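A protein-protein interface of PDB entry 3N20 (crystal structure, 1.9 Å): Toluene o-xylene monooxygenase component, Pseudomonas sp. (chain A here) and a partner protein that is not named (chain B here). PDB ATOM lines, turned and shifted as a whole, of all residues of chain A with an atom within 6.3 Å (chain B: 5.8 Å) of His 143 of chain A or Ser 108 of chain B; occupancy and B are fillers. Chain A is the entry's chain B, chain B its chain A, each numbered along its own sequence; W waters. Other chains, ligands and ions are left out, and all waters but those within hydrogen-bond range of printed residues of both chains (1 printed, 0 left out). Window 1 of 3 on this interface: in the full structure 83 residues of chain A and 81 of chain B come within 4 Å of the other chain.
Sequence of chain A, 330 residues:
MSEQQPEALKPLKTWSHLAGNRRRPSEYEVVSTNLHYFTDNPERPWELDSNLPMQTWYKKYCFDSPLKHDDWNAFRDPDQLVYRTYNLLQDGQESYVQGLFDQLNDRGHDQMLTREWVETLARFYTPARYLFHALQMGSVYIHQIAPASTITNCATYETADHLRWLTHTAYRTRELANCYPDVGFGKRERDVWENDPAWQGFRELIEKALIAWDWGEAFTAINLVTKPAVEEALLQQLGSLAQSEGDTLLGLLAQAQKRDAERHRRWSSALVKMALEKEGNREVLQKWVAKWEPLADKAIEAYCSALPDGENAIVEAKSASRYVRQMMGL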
ATOM      1  N   HIS A  36      11.361 -14.690  -0.678  1.00  0.00           N
ATOM      2  CA  HIS A  36      11.861 -16.054  -0.811  1.00  0.00           C
ATOM      3  C   HIS A  36      12.093 -16.365  -2.278  1.00  0.00           C
ATOM      4  O   HIS A  36      11.242 -16.072  -3.125  1.00  0.00           O
ATOM      5  CB  HIS A  36      10.864 -17.058  -0.225  1.00  0.00           C
ATOM      6  CG  HIS A  36      10.818 -17.055   1.271  1.00  0.00           C
ATOM      7  ND1 HIS A  36       9.756 -17.567   1.989  1.00  0.00           N
ATOM      8  CD2 HIS A  36      11.708 -16.605   2.186  1.00  0.00           C
ATOM      9  CE1 HIS A  36       9.993 -17.430   3.280  1.00  0.00           C
ATOM     10  NE2 HIS A  36      11.171 -16.849   3.428  1.00  0.00           N
ATOM     11  N   GLY A 138       9.529 -24.311  17.932  1.00  0.00           N
ATOM     12  CA  GLY A 138       8.396 -24.595  17.073  1.00  0.00           C
ATOM     13  C   GLY A 138       8.098 -23.503  16.062  1.00  0.00           C
ATOM     14  O   GLY A 138       7.872 -23.786  14.886  1.00  0.00           O
ATOM     15  N   SER A 139       8.105 -22.254  16.508  1.00  0.00           N
ATOM     16  CA  SER A 139       7.811 -21.149  15.609  1.00  0.00           C
ATOM     17  C   SER A 139       8.969 -20.838  14.665  1.00  0.00           C
ATOM     18  O   SER A 139       8.755 -20.340  13.557  1.00  0.00           O
ATOM     19  CB  SER A 139       7.426 -19.890  16.410  1.00  0.00           C
ATOM     20  OG  SER A 139       8.448 -19.501  17.317  1.00  0.00           O
ATOM     21  N   VAL A 140      10.192 -21.143  15.089  1.00  0.00           N
ATOM     22  CA  VAL A 140      11.339 -20.863  14.244  1.00  0.00           C
ATOM     23  C   VAL A 140      11.465 -21.914  13.136  1.00  0.00           C
ATOM     24  O   VAL A 140      12.110 -21.675  12.106  1.00  0.00           O
ATOM     25  CB  VAL A 140      12.652 -20.744  15.083  1.00  0.00           C
ATOM     26  CG1 VAL A 140      13.357 -22.089  15.212  1.00  0.00           C
ATOM     27  CG2 VAL A 140      13.559 -19.693  14.457  1.00  0.00           C
ATOM     28  N   TYR A 141      10.848 -23.076  13.334  1.00  0.00           N
ATOM     29  CA  TYR A 141      10.876 -24.083  12.285  1.00  0.00           C
ATOM     30  C   TYR A 141       9.858 -23.642  11.242  1.00  0.00           C
ATOM     31  O   TYR A 141      10.092 -23.768  10.038  1.00  0.00           O
ATOM     32  CB  TYR A 141      10.510 -25.477  12.792  1.00  0.00           C
ATOM     33  CG  TYR A 141      10.361 -26.445  11.637  1.00  0.00           C
ATOM     34  CD1 TYR A 141       9.102 -26.899  11.235  1.00  0.00           C
ATOM     35  CD2 TYR A 141      11.468 -26.797  10.859  1.00  0.00           C
ATOM     36  CE1 TYR A 141       8.945 -27.669  10.079  1.00  0.00           C
ATOM     37  CE2 TYR A 141      11.323 -27.564   9.700  1.00  0.00           C
ATOM     38  CZ  TYR A 141      10.060 -27.993   9.315  1.00  0.00           C
ATOM     39  OH  TYR A 141       9.915 -28.717   8.150  1.00  0.00           O
ATOM     40  N   ILE A 142       8.728 -23.116  11.707  1.00  0.00           N
ATOM     41  CA  ILE A 142       7.699 -22.637  10.791  1.00  0.00           C
ATOM     42  C   ILE A 142       8.312 -21.576   9.881  1.00  0.00           C
ATOM     43  O   ILE A 142       8.061 -21.546   8.673  1.00  0.00           O
ATOM     44  CB  ILE A 142       6.500 -22.035  11.562  1.00  0.00           C
ATOM     45  CG1 ILE A 142       5.749 -23.158  12.286  1.00  0.00           C
ATOM     46  CG2 ILE A 142       5.567 -21.292  10.600  1.00  0.00           C
ATOM     47  CD1 ILE A 142       4.650 -22.684  13.212  1.00  0.00           C
ATOM     48  N   HIS A 143       9.135 -20.719  10.473  1.00  0.00           N
ATOM     49  CA  HIS A 143       9.814 -19.656   9.739  1.00  0.00           C
ATOM     50  C   HIS A 143      10.559 -20.188   8.508  1.00  0.00           C
ATOM     51  O   HIS A 143      10.371 -19.693   7.389  1.00  0.00           O
ATOM     52  CB  HIS A 143      10.799 -18.939  10.690  1.00  0.00           C
ATOM     53  CG  HIS A 143      11.843 -18.104  10.002  1.00  0.00           C
ATOM     54  ND1 HIS A 143      12.151 -16.822  10.407  1.00  0.00           N
ATOM     55  CD2 HIS A 143      12.689 -18.384   8.981  1.00  0.00           C
ATOM     56  CE1 HIS A 143      13.141 -16.352   9.669  1.00  0.00           C
ATOM     57  NE2 HIS A 143      13.486 -17.281   8.796  1.00  0.00           N
ATOM     58  N   GLN A 144      11.393 -21.203   8.719  1.00  0.00           N
ATOM     59  CA  GLN A 144      12.222 -21.749   7.656  1.00  0.00           C
ATOM     60  C   GLN A 144      11.564 -22.678   6.632  1.00  0.00           C
ATOM     61  O   GLN A 144      12.215 -23.088   5.676  1.00  0.00           O
ATOM     62  CB  GLN A 144      13.448 -22.433   8.287  1.00  0.00           C
ATOM     63  CG  GLN A 144      13.139 -23.722   9.035  1.00  0.00           C
ATOM     64  CD  GLN A 144      14.234 -24.107  10.024  1.00  0.00           C
ATOM     65  OE1 GLN A 144      14.282 -23.597  11.152  1.00  0.00           O
ATOM     66  NE2 GLN A 144      15.122 -25.000   9.603  1.00  0.00           N
ATOM     67  N   ILE A 145      10.281 -22.993   6.800  1.00  0.00           N
ATOM     68  CA  ILE A 145       9.612 -23.883   5.857  1.00  0.00           C
ATOM     69  C   ILE A 145       8.344 -23.274   5.222  1.00  0.00           C
ATOM     70  O   ILE A 145       7.768 -23.866   4.309  1.00  0.00           O
ATOM     71  CB  ILE A 145       9.266 -25.244   6.543  1.00  0.00           C
ATOM     72  CG1 ILE A 145       8.890 -26.300   5.498  1.00  0.00           C
ATOM     73  CG2 ILE A 145       8.129 -25.059   7.537  1.00  0.00           C
ATOM     74  CD1 ILE A 145      10.014 -26.685   4.559  1.00  0.00           C
ATOM     75  N   ALA A 146       7.919 -22.102   5.696  1.00  0.00           N
ATOM     76  CA  ALA A 146       6.733 -21.429   5.141  1.00  0.00           C
ATOM     77  C   ALA A 146       6.988 -21.006   3.685  1.00  0.00           C
ATOM     78  O   ALA A 146       8.101 -20.613   3.330  1.00  0.00           O
ATOM     79  CB  ALA A 146       6.370 -20.202   5.991  1.00  0.00           C
ATOM     80  N   ALA A 148       6.039 -18.291   1.948  1.00  0.00           N
ATOM     81  CA  ALA A 148       6.088 -16.869   1.598  1.00  0.00           C
ATOM     82  C   ALA A 148       6.817 -16.063   2.667  1.00  0.00           C
ATOM     83  O   ALA A 148       6.691 -16.355   3.855  1.00  0.00           O
ATOM     84  CB  ALA A 148       4.661 -16.326   1.406  1.00  0.00           C
ATOM     85  N   ILE A 151       4.691 -14.705   5.560  1.00  0.00           N
ATOM     86  CA  ILE A 151       4.269 -15.695   6.549  1.00  0.00           C
ATOM     87  C   ILE A 151       5.465 -15.923   7.470  1.00  0.00           C
ATOM     88  O   ILE A 151       5.337 -15.940   8.689  1.00  0.00           O
ATOM     89  CB  ILE A 151       3.903 -17.045   5.888  1.00  0.00           C
ATOM     90  CG1 ILE A 151       2.711 -16.865   4.951  1.00  0.00           C
ATOM     91  CG2 ILE A 151       3.571 -18.087   6.955  1.00  0.00           C
ATOM     92  CD1 ILE A 151       2.354 -18.133   4.197  1.00  0.00           C
ATOM     93  N   THR A 152       6.632 -16.095   6.853  1.00  0.00           N
ATOM     94  CA  THR A 152       7.877 -16.314   7.580  1.00  0.00           C
ATOM     95  C   THR A 152       8.167 -15.226   8.609  1.00  0.00           C
ATOM     96  O   THR A 152       8.580 -15.526   9.731  1.00  0.00           O
ATOM     97  CB  THR A 152       9.073 -16.399   6.600  1.00  0.00           C
ATOM     98  OG1 THR A 152       9.031 -17.653   5.913  1.00  0.00           O
ATOM     99  CG2 THR A 152      10.408 -16.256   7.341  1.00  0.00           C
ATOM    100  N   ASN A 153       7.959 -13.966   8.230  1.00  0.00           N
ATOM    101  CA  ASN A 153       8.221 -12.858   9.141  1.00  0.00           C
ATOM    102  C   ASN A 153       7.347 -12.894  10.387  1.00  0.00           C
ATOM    103  O   ASN A 153       7.825 -12.615  11.494  1.00  0.00           O
ATOM    104  CB  ASN A 153       8.069 -11.519   8.416  1.00  0.00           C
ATOM    105  CG  ASN A 153       9.236 -11.226   7.491  1.00  0.00           C
ATOM    106  OD1 ASN A 153       9.327 -10.147   6.907  1.00  0.00           O
ATOM    107  ND2 ASN A 153      10.140 -12.193   7.353  1.00  0.00           N
ATOM    108  N   ALA A 155       6.305 -15.453  11.785  1.00  0.00           N
ATOM    109  CA  ALA A 155       6.903 -16.519  12.590  1.00  0.00           C
ATOM    110  C   ALA A 155       8.222 -16.047  13.209  1.00  0.00           C
ATOM    111  O   ALA A 155       8.600 -16.486  14.296  1.00  0.00           O
ATOM    112  CB  ALA A 155       7.140 -17.770  11.728  1.00  0.00           C
ATOM    113  N   THR A 156       8.915 -15.155  12.505  1.00  0.00           N
ATOM    114  CA  THR A 156      10.177 -14.600  12.979  1.00  0.00           C
ATOM    115  C   THR A 156       9.956 -13.844  14.289  1.00  0.00           C
ATOM    116  O   THR A 156      10.592 -14.129  15.305  1.00  0.00           O
ATOM    117  CB  THR A 156      10.779 -13.605  11.953  1.00  0.00           C
ATOM    118  OG1 THR A 156      10.979 -14.261  10.694  1.00  0.00           O
ATOM    119  CG2 THR A 156      12.111 -13.065  12.456  1.00  0.00           C
ATOM    120  N   THR A 159       8.770 -15.937  17.146  1.00  0.00           N
ATOM    121  CA  THR A 159       9.882 -16.678  17.735  1.00  0.00           C
ATOM    122  C   THR A 159      10.606 -15.784  18.737  1.00  0.00           C
ATOM    123  O   THR A 159      10.976 -16.227  19.827  1.00  0.00           O
ATOM    124  CB  THR A 159      10.872 -17.158  16.642  1.00  0.00           C
ATOM    125  OG1 THR A 159      10.194 -18.059  15.760  1.00  0.00           O
ATOM    126  CG2 THR A 159      12.060 -17.885  17.258  1.00  0.00           C
ATOM    127  N   GLU B 103      19.757 -12.031  -0.085  1.00  0.00           N
ATOM    128  CA  GLU B 103      20.576 -13.089   0.490  1.00  0.00           C
ATOM    129  C   GLU B 103      20.704 -12.809   1.985  1.00  0.00           C
ATOM    130  O   GLU B 103      20.782 -13.735   2.795  1.00  0.00           O
ATOM    131  CB  GLU B 103      21.945 -13.142  -0.192  1.00  0.00           C
ATOM    132  CG  GLU B 103      21.882 -13.635  -1.645  1.00  0.00           C
ATOM    133  CD  GLU B 103      21.475 -15.103  -1.772  1.00  0.00           C
ATOM    134  OE1 GLU B 103      20.857 -15.651  -0.835  1.00  0.00           O
ATOM    135  OE2 GLU B 103      21.760 -15.719  -2.823  1.00  0.00           O
ATOM    136  N   GLU B 104      20.707 -11.529   2.353  1.00  0.00           N
ATOM    137  CA  GLU B 104      20.757 -11.146   3.763  1.00  0.00           C
ATOM    138  C   GLU B 104      19.491 -11.708   4.411  1.00  0.00           C
ATOM    139  O   GLU B 104      19.536 -12.330   5.479  1.00  0.00           O
ATOM    140  CB  GLU B 104      20.764  -9.616   3.910  1.00  0.00           C
ATOM    141  CG  GLU B 104      22.090  -8.953   3.560  1.00  0.00           C
ATOM    142  CD  GLU B 104      22.977  -8.753   4.771  1.00  0.00           C
ATOM    143  OE1 GLU B 104      22.939  -9.601   5.684  1.00  0.00           O
ATOM    144  OE2 GLU B 104      23.720  -7.752   4.814  1.00  0.00           O
ATOM    145  N   TYR B 105      18.355 -11.489   3.751  1.00  0.00           N
ATOM    146  CA  TYR B 105      17.082 -11.972   4.269  1.00  0.00           C
ATOM    147  C   TYR B 105      17.060 -13.494   4.333  1.00  0.00           C
ATOM    148  O   TYR B 105      16.496 -14.078   5.260  1.00  0.00           O
ATOM    149  CB  TYR B 105      15.922 -11.491   3.399  1.00  0.00           C
ATOM    150  CG  TYR B 105      14.584 -12.011   3.877  1.00  0.00           C
ATOM    151  CD1 TYR B 105      13.996 -11.517   5.044  1.00  0.00           C
ATOM    152  CD2 TYR B 105      13.931 -13.028   3.192  1.00  0.00           C
ATOM    153  CE1 TYR B 105      12.789 -12.029   5.512  1.00  0.00           C
ATOM    154  CE2 TYR B 105      12.728 -13.546   3.648  1.00  0.00           C
ATOM    155  CZ  TYR B 105      12.159 -13.045   4.806  1.00  0.00           C
ATOM    156  OH  TYR B 105      10.958 -13.564   5.242  1.00  0.00           O
ATOM    157  N   ALA B 106      17.665 -14.136   3.339  1.00  0.00           N
ATOM    158  CA  ALA B 106      17.724 -15.590   3.310  1.00  0.00           C
ATOM    159  C   ALA B 106      18.540 -16.100   4.497  1.00  0.00           C
ATOM    160  O   ALA B 106      18.280 -17.185   5.014  1.00  0.00           O
ATOM    161  CB  ALA B 106      18.343 -16.070   1.995  1.00  0.00           C
ATOM    162  N   ALA B 107      19.523 -15.313   4.930  1.00  0.00           N
ATOM    163  CA  ALA B 107      20.363 -15.706   6.059  1.00  0.00           C
ATOM    164  C   ALA B 107      19.570 -15.859   7.356  1.00  0.00           C
ATOM    165  O   ALA B 107      20.020 -16.546   8.279  1.00  0.00           O
ATOM    166  CB  ALA B 107      21.491 -14.703   6.247  1.00  0.00           C
ATOM    167  N   SER B 108      18.393 -15.237   7.441  1.00  0.00           N
ATOM    168  CA  SER B 108      17.590 -15.382   8.654  1.00  0.00           C
ATOM    169  C   SER B 108      17.084 -16.822   8.723  1.00  0.00           C
ATOM    170  O   SER B 108      16.868 -17.358   9.812  1.00  0.00           O
ATOM    171  CB  SER B 108      16.413 -14.388   8.681  1.00  0.00           C
ATOM    172  OG  SER B 108      15.513 -14.610   7.611  1.00  0.00           O
ATOM    173  N   THR B 109      16.912 -17.453   7.562  1.00  0.00           N
ATOM    174  CA  THR B 109      16.474 -18.850   7.514  1.00  0.00           C
ATOM    175  C   THR B 109      17.666 -19.736   7.892  1.00  0.00           C
ATOM    176  O   THR B 109      17.508 -20.757   8.568  1.00  0.00           O
ATOM    177  CB  THR B 109      15.953 -19.244   6.102  1.00  0.00           C
ATOM    178  OG1 THR B 109      14.676 -18.631   5.876  1.00  0.00           O
ATOM    179  CG2 THR B 109      15.801 -20.762   5.975  1.00  0.00           C
ATOM    180  N   ALA B 110      18.861 -19.338   7.457  1.00  0.00           N
ATOM    181  CA  ALA B 110      20.069 -20.086   7.790  1.00  0.00           C
ATOM    182  C   ALA B 110      20.220 -20.050   9.315  1.00  0.00           C
ATOM    183  O   ALA B 110      20.600 -21.046   9.942  1.00  0.00           O
ATOM    184  CB  ALA B 110      21.283 -19.450   7.119  1.00  0.00           C
ATOM    185  N   GLU B 111      19.907 -18.896   9.908  1.00  0.00           N
ATOM    186  CA  GLU B 111      19.990 -18.726  11.361  1.00  0.00           C
ATOM    187  C   GLU B 111      18.890 -19.560  12.022  1.00  0.00           C
ATOM    188  O   GLU B 111      19.111 -20.205  13.046  1.00  0.00           O
ATOM    189  CB  GLU B 111      19.836 -17.247  11.747  1.00  0.00           C
ATOM    190  CG  GLU B 111      21.041 -16.362  11.422  1.00  0.00           C
ATOM    191  CD  GLU B 111      22.240 -16.589  12.356  1.00  0.00           C
ATOM    192  OE1 GLU B 111      22.060 -17.177  13.445  1.00  0.00           O
ATOM    193  OE2 GLU B 111      23.367 -16.160  12.011  1.00  0.00           O
ATOM    194  N   ALA B 112      17.708 -19.556  11.415  1.00  0.00           N
ATOM    195  CA  ALA B 112      16.585 -20.328  11.933  1.00  0.00           C
ATOM    196  C   ALA B 112      16.927 -21.820  11.924  1.00  0.00           C
ATOM    197  O   ALA B 112      16.449 -22.576  12.769  1.00  0.00           O
ATOM    198  CB  ALA B 112      15.333 -20.064  11.086  1.00  0.00           C
ATOM    199  N   ARG B 113      17.743 -22.250  10.964  1.00  0.00           N
ATOM    200  CA  ARG B 113      18.134 -23.657  10.891  1.00  0.00           C
ATOM    201  C   ARG B 113      18.852 -24.024  12.201  1.00  0.00           C
ATOM    202  O   ARG B 113      18.612 -25.086  12.787  1.00  0.00           O
ATOM    203  CB  ARG B 113      19.073 -23.897   9.697  1.00  0.00           C
ATOM    204  CG  ARG B 113      19.183 -25.368   9.273  1.00  0.00           C
ATOM    205  CD  ARG B 113      17.993 -25.786   8.411  1.00  0.00           C
ATOM    206  NE  ARG B 113      18.092 -25.241   7.057  1.00  0.00           N
ATOM    207  CZ  ARG B 113      17.053 -24.849   6.323  1.00  0.00           C
ATOM    208  NH1 ARG B 113      15.819 -24.931   6.813  1.00  0.00           N
ATOM    209  NH2 ARG B 113      17.246 -24.387   5.094  1.00  0.00           N
ATOM    210  N   ALA B 127      21.275 -17.864  17.706  1.00  0.00           N
ATOM    211  CA  ALA B 127      20.799 -17.950  16.328  1.00  0.00           C
ATOM    212  C   ALA B 127      19.424 -17.295  16.223  1.00  0.00           C
ATOM    213  O   ALA B 127      19.003 -16.889  15.145  1.00  0.00           O
ATOM    214  CB  ALA B 127      20.729 -19.413  15.871  1.00  0.00           C
ATOM    215  N   GLY B 130      20.385 -13.899  15.845  1.00  0.00           N
ATOM    216  CA  GLY B 130      20.973 -13.820  14.524  1.00  0.00           C
ATOM    217  C   GLY B 130      19.887 -13.803  13.467  1.00  0.00           C
ATOM    218  O   GLY B 130      20.015 -13.145  12.434  1.00  0.00           O
ATOM    219  N   MET B 131      18.818 -14.549  13.722  1.00  0.00           N
ATOM    220  CA  MET B 131      17.693 -14.609  12.803  1.00  0.00           C
ATOM    221  C   MET B 131      17.078 -13.211  12.698  1.00  0.00           C
ATOM    222  O   MET B 131      16.744 -12.747  11.603  1.00  0.00           O
ATOM    223  CB  MET B 131      16.651 -15.604  13.313  1.00  0.00           C
ATOM    224  CG  MET B 131      15.316 -15.510  12.599  1.00  0.00           C
ATOM    225  SD  MET B 131      14.004 -16.323  13.527  1.00  0.00           S
ATOM    226  CE  MET B 131      13.807 -15.187  14.914  1.00  0.00           C
ATOM    227  N   MET B 132      16.938 -12.546  13.845  1.00  0.00           N
ATOM    228  CA  MET B 132      16.389 -11.192  13.886  1.00  0.00           C
ATOM    229  C   MET B 132      17.319 -10.211  13.181  1.00  0.00           C
ATOM    230  O   MET B 132      16.856  -9.317  12.463  1.00  0.00           O
ATOM    231  CB  MET B 132      16.155 -10.746  15.335  1.00  0.00           C
ATOM    232  CG  MET B 132      14.909 -11.349  15.973  1.00  0.00           C
ATOM    233  SD  MET B 132      13.377 -10.732  15.201  1.00  0.00           S
ATOM    234  CE  MET B 132      13.220  -9.132  16.044  1.00  0.00           C
ATOM    235  N   GLU B 134      19.463 -10.713  10.619  1.00  0.00           N
ATOM    236  CA  GLU B 134      19.390 -10.812   9.168  1.00  0.00           C
ATOM    237  C   GLU B 134      18.035 -10.319   8.662  1.00  0.00           C
ATOM    238  O   GLU B 134      17.907  -9.899   7.510  1.00  0.00           O
ATOM    239  CB  GLU B 134      19.646 -12.252   8.723  1.00  0.00           C
ATOM    240  CG  GLU B 134      20.946 -12.856   9.272  1.00  0.00           C
ATOM    241  CD  GLU B 134      22.201 -12.095   8.865  1.00  0.00           C
ATOM    242  OE1 GLU B 134      22.095 -11.031   8.216  1.00  0.00           O
ATOM    243  OE2 GLU B 134      23.312 -12.565   9.199  1.00  0.00           O
ATOM    244  N   ASN B 135      17.021 -10.381   9.520  1.00  0.00           N
ATOM    245  CA  ASN B 135      15.699  -9.878   9.151  1.00  0.00           C
ATOM    246  C   ASN B 135      15.886  -8.364   9.002  1.00  0.00           C
ATOM    247  O   ASN B 135      15.420  -7.756   8.032  1.00  0.00           O
ATOM    248  CB  ASN B 135      14.675 -10.203  10.252  1.00  0.00           C
ATOM    249  CG  ASN B 135      13.290  -9.604   9.983  1.00  0.00           C
ATOM    250  OD1 ASN B 135      12.984  -8.485  10.406  1.00  0.00           O
ATOM    251  ND2 ASN B 135      12.449 -10.354   9.276  1.00  0.00           N
HETATM  252  O   HOH W   1      12.846 -13.023   8.798  1.00  0.00           O
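The backbone carbonyl oxygen of Ala 155 of chain A lies within hydrogen-bond range of the side-chain hydroxyl of Thr 159 of chain A (2.7 Å). NE2 of His 36 of chain A lies close to OG1 of Thr 152 of chain A (3.4 Å). The backbone carbonyl oxygen (O) of Val 140 of chain A sits close to the side-chain amide oxygen (OE1) of Gln 144 of chain A (3.1 Å). The backbone carbonyl oxygen (O) of Thr 152 of chain A sits at hydrogen-bond distance from the side-chain hydroxyl (OG1) of Thr 156 of chain A (2.9 Å). The side-chain hydroxyl of Thr 152 of chain A sits at hydrogen-bond distance from the backbone carbonyl oxygen of His 143 of chain A, at 2.9 Å. The backbone NH (N) of Val 140 of chain A sits at hydrogen-bond distance from the side-chain hydroxyl (OG1) of Thr 159 of chain A (3.2 Å).
A ring nitrogen (ND1) of His 143 of chain A is in hydrogen-bond range of the side-chain sulfur (SD) of Met 131 of chain B (3.7 Å). The side-chain amide oxygen of Gln 144 of chain A lies close to the backbone carbonyl oxygen of Ala 112 of chain B, at 2.9 Å. OH of Tyr 105 of chain B sits at hydrogen-bond distance from ND2 of Asn 153 of chain A, 2.6 Å away. The side-chain amide nitrogen (NE2) of Gln 144 of chain A lies close to the guanidinium group (NH1) of Arg 113 of chain B (2.9 Å). NE2 of His 143 of chain A lies within hydrogen-bond range of OG1 of Thr 109 of chain B (3.4 Å).
Of the 17 printed residues of chain B, 8 touch a printed residue of chain A. Hydrophobic or aromatic side chains of chain B that line the printed part of chain A: Tyr 105, Ala 112, Met 131 and Met 132. Along chain B the printed residues that touch a printed residue of chain A span positions 105 to 135. Along chain A the printed residues that touch a printed residue of chain B span positions 36 to 159. Among the printed residues, 16 pairs touch across the chains.
Water W1 lies within hydrogen-bond range of ND2 of Asn 135 of chain B, OG1 of Thr 156 of chain A, ND2 of Asn 153 of chain A and OG of Ser 108 of chain B.
Among the printed residues, pairs that only touch across the chains: Thr 156 of chain A with Met 131 of chain B (3.4 Å), Thr 152 of chain A with Tyr 105 of chain B (3.5 Å), Asn 153 of chain A with Asn 135 of chain B (3.5 Å), Val 140 of chain A with Met 131 of chain B (3.5 Å), His 143 of chain A with Ser 108 of chain B (3.5 Å), His 36 of chain A with Tyr 105 of chain B (3.5 Å), Gln 144 of chain A with Thr 109 of chain B (3.7 Å), Val 140 of chain A with Ala 112 of chain B (3.7 Å), His 143 of chain A with Ala 112 of chain B (3.8 Å), Thr 156 of chain A with Met 132 of chain B (3.8 Å) and Thr 159 of chain A with Met 131 of chain B (3.9 Å).
His 143 of chain A touches just these residues of chain B: Ser 108 (3.5 Å), Thr 109 (3.4 Å), Ala 112 (3.8 Å) and Met 131 (3.7 Å). Ser 108 of chain B touches one residue of chain A. Of the printed residues of chain A, Asn 135 of chain B touches Asn 153. Of the printed residues of chain A, Ala 112 of chain B touches Val 140, His 143 and Gln 144. Printed residues of chain B within 4 Å of Thr 152 of chain A: Tyr 105. Printed residues of chain A within 4 Å of Met 131 of chain B: Val 140, His 143, Thr 156 and Thr 159. The nearest residue of chain B that does not touch His 143 of chain A is Tyr 105 of chain B (5.6 Å).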
